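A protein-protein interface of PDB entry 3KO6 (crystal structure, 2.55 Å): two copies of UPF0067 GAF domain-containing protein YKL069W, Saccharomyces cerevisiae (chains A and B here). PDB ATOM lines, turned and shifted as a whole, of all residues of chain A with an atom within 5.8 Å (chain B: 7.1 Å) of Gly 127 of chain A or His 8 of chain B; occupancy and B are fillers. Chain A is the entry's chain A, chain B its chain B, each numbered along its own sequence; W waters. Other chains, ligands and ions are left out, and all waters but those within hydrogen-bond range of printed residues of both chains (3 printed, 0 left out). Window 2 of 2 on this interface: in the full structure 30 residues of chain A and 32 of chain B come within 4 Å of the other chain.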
ATOM      1  N   ASN A 117      35.807  25.000 -32.134  1.00  0.00           N
ATOM      2  CA  ASN A 117      36.376  23.705 -32.415  1.00  0.00           C
ATOM      3  C   ASN A 117      37.791  23.811 -32.992  1.00  0.00           C
ATOM      4  O   ASN A 117      38.541  22.833 -32.949  1.00  0.00           O
ATOM      5  CB  ASN A 117      35.433  22.896 -33.305  1.00  0.00           C
ATOM      6  CG  ASN A 117      34.059  22.693 -32.654  1.00  0.00           C
ATOM      7  OD1 ASN A 117      33.962  22.223 -31.514  1.00  0.00           O
ATOM      8  ND2 ASN A 117      33.000  23.061 -33.372  1.00  0.00           N
ATOM      9  N   ALA A 124      34.301  23.019 -23.903  1.00  0.00           N
ATOM     10  CA  ALA A 124      32.932  23.021 -24.387  1.00  0.00           C
ATOM     11  C   ALA A 124      31.993  22.597 -23.277  1.00  0.00           C
ATOM     12  O   ALA A 124      32.020  21.454 -22.829  1.00  0.00           O
ATOM     13  CB  ALA A 124      32.775  22.127 -25.617  1.00  0.00           C
ATOM     14  N   CYS A 125      31.183  23.535 -22.803  1.00  0.00           N
ATOM     15  CA  CYS A 125      30.160  23.197 -21.822  1.00  0.00           C
ATOM     16  C   CYS A 125      28.870  22.832 -22.540  1.00  0.00           C
ATOM     17  O   CYS A 125      28.064  22.053 -22.037  1.00  0.00           O
ATOM     18  CB  CYS A 125      29.966  24.323 -20.816  1.00  0.00           C
ATOM     19  SG  CYS A 125      31.492  24.842 -20.029  1.00  0.00           S
ATOM     20  N   ASP A 126      28.709  23.392 -23.736  1.00  0.00           N
ATOM     21  CA  ASP A 126      27.601  23.083 -24.623  1.00  0.00           C
ATOM     22  C   ASP A 126      28.210  22.665 -25.959  1.00  0.00           C
ATOM     23  O   ASP A 126      28.920  23.442 -26.595  1.00  0.00           O
ATOM     24  CB  ASP A 126      26.684  24.304 -24.770  1.00  0.00           C
ATOM     25  CG  ASP A 126      25.452  24.033 -25.621  1.00  0.00           C
ATOM     26  OD1 ASP A 126      25.399  23.036 -26.370  1.00  0.00           O
ATOM     27  OD2 ASP A 126      24.511  24.846 -25.544  1.00  0.00           O
ATOM     28  N   GLY A 127      27.944  21.430 -26.371  1.00  0.00           N
ATOM     29  CA  GLY A 127      28.528  20.911 -27.597  1.00  0.00           C
ATOM     30  C   GLY A 127      28.135  21.642 -28.873  1.00  0.00           C
ATOM     31  O   GLY A 127      28.853  21.579 -29.869  1.00  0.00           O
ATOM     32  N   GLU A 128      27.001  22.343 -28.844  1.00  0.00           N
ATOM     33  CA  GLU A 128      26.477  23.002 -30.052  1.00  0.00           C
ATOM     34  C   GLU A 128      27.095  24.384 -30.315  1.00  0.00           C
ATOM     35  O   GLU A 128      26.919  24.955 -31.398  1.00  0.00           O
ATOM     36  CB  GLU A 128      24.950  23.094 -29.997  1.00  0.00           C
ATOM     37  CG  GLU A 128      24.217  21.754 -30.077  1.00  0.00           C
ATOM     38  CD  GLU A 128      22.706  21.905 -29.897  1.00  0.00           C
ATOM     39  OE1 GLU A 128      22.217  23.065 -29.741  1.00  0.00           O
ATOM     40  OE2 GLU A 128      22.007  20.856 -29.911  1.00  0.00           O
ATOM     41  N   THR A 129      27.830  24.898 -29.332  1.00  0.00           N
ATOM     42  CA  THR A 129      28.488  26.202 -29.427  1.00  0.00           C
ATOM     43  C   THR A 129      29.508  26.217 -30.540  1.00  0.00           C
ATOM     44  O   THR A 129      30.410  25.378 -30.544  1.00  0.00           O
ATOM     45  CB  THR A 129      29.224  26.545 -28.122  1.00  0.00           C
ATOM     46  OG1 THR A 129      28.293  26.589 -27.031  1.00  0.00           O
ATOM     47  CG2 THR A 129      29.922  27.878 -28.245  1.00  0.00           C
ATOM     48  N   SER B   4      36.900  10.647 -23.755  1.00  0.00           N
ATOM     49  CA  SER B   4      35.757  11.599 -23.600  1.00  0.00           C
ATOM     50  C   SER B   4      34.422  10.888 -23.769  1.00  0.00           C
ATOM     51  O   SER B   4      34.219  10.134 -24.719  1.00  0.00           O
ATOM     52  CB  SER B   4      35.867  12.785 -24.582  1.00  0.00           C
ATOM     53  OG  SER B   4      34.678  13.594 -24.610  1.00  0.00           O
ATOM     54  N   THR B   5      33.516  11.178 -22.843  1.00  0.00           N
ATOM     55  CA  THR B   5      32.205  10.537 -22.758  1.00  0.00           C
ATOM     56  C   THR B   5      31.271  10.878 -23.915  1.00  0.00           C
ATOM     57  O   THR B   5      30.250  10.233 -24.099  1.00  0.00           O
ATOM     58  CB  THR B   5      31.485  10.965 -21.469  1.00  0.00           C
ATOM     59  OG1 THR B   5      31.373  12.398 -21.440  1.00  0.00           O
ATOM     60  CG2 THR B   5      32.246  10.490 -20.239  1.00  0.00           C
ATOM     61  N   GLY B   6      31.594  11.918 -24.670  1.00  0.00           N
ATOM     62  CA  GLY B   6      30.693  12.389 -25.711  1.00  0.00           C
ATOM     63  C   GLY B   6      29.483  13.106 -25.137  1.00  0.00           C
ATOM     64  O   GLY B   6      28.528  13.409 -25.854  1.00  0.00           O
ATOM     65  N   PHE B   7      29.522  13.362 -23.837  1.00  0.00           N
ATOM     66  CA  PHE B   7      28.479  14.123 -23.187  1.00  0.00           C
ATOM     67  C   PHE B   7      29.023  15.504 -22.887  1.00  0.00           C
ATOM     68  O   PHE B   7      30.214  15.662 -22.600  1.00  0.00           O
ATOM     69  CB  PHE B   7      28.079  13.472 -21.870  1.00  0.00           C
ATOM     70  CG  PHE B   7      27.153  12.306 -22.007  1.00  0.00           C
ATOM     71  CD1 PHE B   7      27.579  11.025 -21.668  1.00  0.00           C
ATOM     72  CD2 PHE B   7      25.848  12.482 -22.435  1.00  0.00           C
ATOM     73  CE1 PHE B   7      26.716   9.935 -21.759  1.00  0.00           C
ATOM     74  CE2 PHE B   7      24.985  11.404 -22.542  1.00  0.00           C
ATOM     75  CZ  PHE B   7      25.425  10.122 -22.200  1.00  0.00           C
ATOM     76  N   HIS B   8      28.160  16.509 -22.961  1.00  0.00           N
ATOM     77  CA  HIS B   8      28.523  17.843 -22.473  1.00  0.00           C
ATOM     78  C   HIS B   8      27.652  18.213 -21.290  1.00  0.00           C
ATOM     79  O   HIS B   8      26.593  17.601 -21.075  1.00  0.00           O
ATOM     80  CB  HIS B   8      28.476  18.898 -23.593  1.00  0.00           C
ATOM     81  CG  HIS B   8      29.490  18.663 -24.674  1.00  0.00           C
ATOM     82  ND1 HIS B   8      29.171  18.094 -25.887  1.00  0.00           N
ATOM     83  CD2 HIS B   8      30.827  18.878 -24.702  1.00  0.00           C
ATOM     84  CE1 HIS B   8      30.259  17.995 -26.628  1.00  0.00           C
ATOM     85  NE2 HIS B   8      31.278  18.467 -25.934  1.00  0.00           N
ATOM     86  N   HIS B   9      28.120  19.188 -20.508  1.00  0.00           N
ATOM     87  CA  HIS B   9      27.362  19.719 -19.375  1.00  0.00           C
ATOM     88  C   HIS B   9      25.942  20.072 -19.777  1.00  0.00           C
ATOM     89  O   HIS B   9      24.996  19.769 -19.038  1.00  0.00           O
ATOM     90  CB  HIS B   9      28.043  20.946 -18.787  1.00  0.00           C
ATOM     91  CG  HIS B   9      29.126  20.626 -17.809  1.00  0.00           C
ATOM     92  ND1 HIS B   9      30.408  20.305 -18.199  1.00  0.00           N
ATOM     93  CD2 HIS B   9      29.125  20.595 -16.455  1.00  0.00           C
ATOM     94  CE1 HIS B   9      31.148  20.078 -17.128  1.00  0.00           C
ATOM     95  NE2 HIS B   9      30.396  20.255 -16.057  1.00  0.00           N
ATOM     96  N   ALA B  10      25.798  20.692 -20.947  1.00  0.00           N
ATOM     97  CA  ALA B  10      24.491  21.101 -21.472  1.00  0.00           C
ATOM     98  C   ALA B  10      23.507  19.949 -21.656  1.00  0.00           C
ATOM     99  O   ALA B  10      22.301  20.164 -21.626  1.00  0.00           O
ATOM    100  CB  ALA B  10      24.665  21.846 -22.771  1.00  0.00           C
ATOM    101  N   ASP B  11      24.031  18.728 -21.813  1.00  0.00           N
ATOM    102  CA  ASP B  11      23.210  17.540 -22.050  1.00  0.00           C
ATOM    103  C   ASP B  11      22.219  17.239 -20.932  1.00  0.00           C
ATOM    104  O   ASP B  11      21.212  16.582 -21.166  1.00  0.00           O
ATOM    105  CB  ASP B  11      24.071  16.317 -22.375  1.00  0.00           C
ATOM    106  CG  ASP B  11      24.747  16.424 -23.729  1.00  0.00           C
ATOM    107  OD1 ASP B  11      25.800  15.794 -23.925  1.00  0.00           O
ATOM    108  OD2 ASP B  11      24.244  17.152 -24.603  1.00  0.00           O
ATOM    109  N   HIS B  12      22.480  17.751 -19.735  1.00  0.00           N
ATOM    110  CA  HIS B  12      21.563  17.545 -18.620  1.00  0.00           C
ATOM    111  C   HIS B  12      20.162  18.074 -18.865  1.00  0.00           C
ATOM    112  O   HIS B  12      19.229  17.620 -18.216  1.00  0.00           O
ATOM    113  CB  HIS B  12      22.115  18.146 -17.345  1.00  0.00           C
ATOM    114  CG  HIS B  12      23.170  17.309 -16.706  1.00  0.00           C
ATOM    115  ND1 HIS B  12      22.874  16.234 -15.900  1.00  0.00           N
ATOM    116  CD2 HIS B  12      24.519  17.379 -16.761  1.00  0.00           C
ATOM    117  CE1 HIS B  12      23.997  15.680 -15.482  1.00  0.00           C
ATOM    118  NE2 HIS B  12      25.009  16.354 -15.993  1.00  0.00           N
ATOM    119  N   VAL B  13      20.021  19.029 -19.785  1.00  0.00           N
ATOM    120  CA  VAL B  13      18.710  19.620 -20.104  1.00  0.00           C
ATOM    121  C   VAL B  13      18.267  19.305 -21.521  1.00  0.00           C
ATOM    122  O   VAL B  13      17.327  19.917 -22.037  1.00  0.00           O
ATOM    123  CB  VAL B  13      18.667  21.154 -19.919  1.00  0.00           C
ATOM    124  CG1 VAL B  13      19.036  21.547 -18.492  1.00  0.00           C
ATOM    125  CG2 VAL B  13      19.531  21.856 -20.942  1.00  0.00           C
ATOM    126  N   ASN B  14      18.959  18.366 -22.154  1.00  0.00           N
ATOM    127  CA  ASN B  14      18.503  17.850 -23.426  1.00  0.00           C
ATOM    128  C   ASN B  14      17.554  16.651 -23.188  1.00  0.00           C
ATOM    129  O   ASN B  14      17.875  15.515 -23.510  1.00  0.00           O
ATOM    130  CB  ASN B  14      19.692  17.574 -24.376  1.00  0.00           C
ATOM    131  CG  ASN B  14      20.484  18.872 -24.750  1.00  0.00           C
ATOM    132  OD1 ASN B  14      19.908  19.954 -24.940  1.00  0.00           O
ATOM    133  ND2 ASN B  14      21.804  18.747 -24.862  1.00  0.00           N
HETATM  134  O   HOH W   1      23.350  21.339 -26.414  1.00  0.00           O
HETATM  135  O   HOH W   2      30.836  19.691 -20.817  1.00  0.00           O
HETATM  136  O   HOH W   3      25.721  19.570 -25.576  1.00  0.00           O
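The backbone carbonyl oxygen (O) of Cys 125 of chain A is in hydrogen-bond range of the backbone NH (N) of His 9 of chain B, 3.2 Å away. O of Cys 125 of chain A lies within hydrogen-bond range of N of Ala 10 of chain B (2.9 Å).
The side-chain carboxylate (OD1) of Asp 126 of chain A sits at hydrogen-bond distance from the backbone NH (N) of Glu 128 of chain A (3.0 Å). O of Asp 126 of chain A lies within hydrogen-bond range of OG1 of Thr 129 of chain A (3.2 Å). N of His 8 of chain B sits at hydrogen-bond distance from OD1 of Asp 11 of chain B.
Ala 124 of chain A touches His 8 of chain B (O to CD2, 3.4 Å). CB of His 8 of chain B touches O of Cys 125 of chain A (3.5 Å). Asp 126 of chain A touches Ala 10 of chain B (CG to CB, 3.7 Å). His 8 of chain B touches Gly 127 of chain A (ND1 to CA, 3.4 Å).
Printed residues of chain B within 4 Å of Ala 124 of chain A: His 8. Of the printed residues of chain B, Cys 125 of chain A touches His 8 (3.5 Å), His 9 (3.2 Å) and Ala 10 (2.9 Å). Of the printed residues of chain B, Asp 126 of chain A touches Ala 10. Of chain B, only His 8 (3.4 Å) comes within 4 Å of Gly 127 of chain A. Gly 6 of chain B touches none of the printed residues of chain A. Of chain A, only Ala 124, Cys 125 and Gly 127 come within 4 Å of His 8 of chain B. Printed residues of chain A within 4 Å of His 9 of chain B: Cys 125 (3.2 Å). Of the printed residues of chain A, Ala 10 of chain B touches Cys 125 and Asp 126. The nearest printed residue of chain B that does not touch Asp 126 of chain A is His 8 of chain B (4.4 Å).
Hydrophobic or aromatic side chains of chain B that line the printed part of chain A: His 8, His 9 and Ala 10. Printed residues of chain A that touch a printed residue of chain B: Ala 124, Cys 125, Asp 126 and Gly 127. Hydrophobic or aromatic side chains of chain A that line the printed part of chain B: Ala 124.
No position is printed for both chains.
Water W1 bridges OD1 of Asp 126 of chain A and ND2 of Asn 14 of chain B. Water W2 bridges a ring nitrogen (ND1) of His 9 of chain B (2.7 Å) and the backbone carbonyl oxygen (O) of Ala 124 of chain A (2.9 Å). Water W3 lies within hydrogen-bond range of OD2 of Asp 11 of chain B (3.0 Å) and N of Gly 127 of chain A (3.0 Å).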
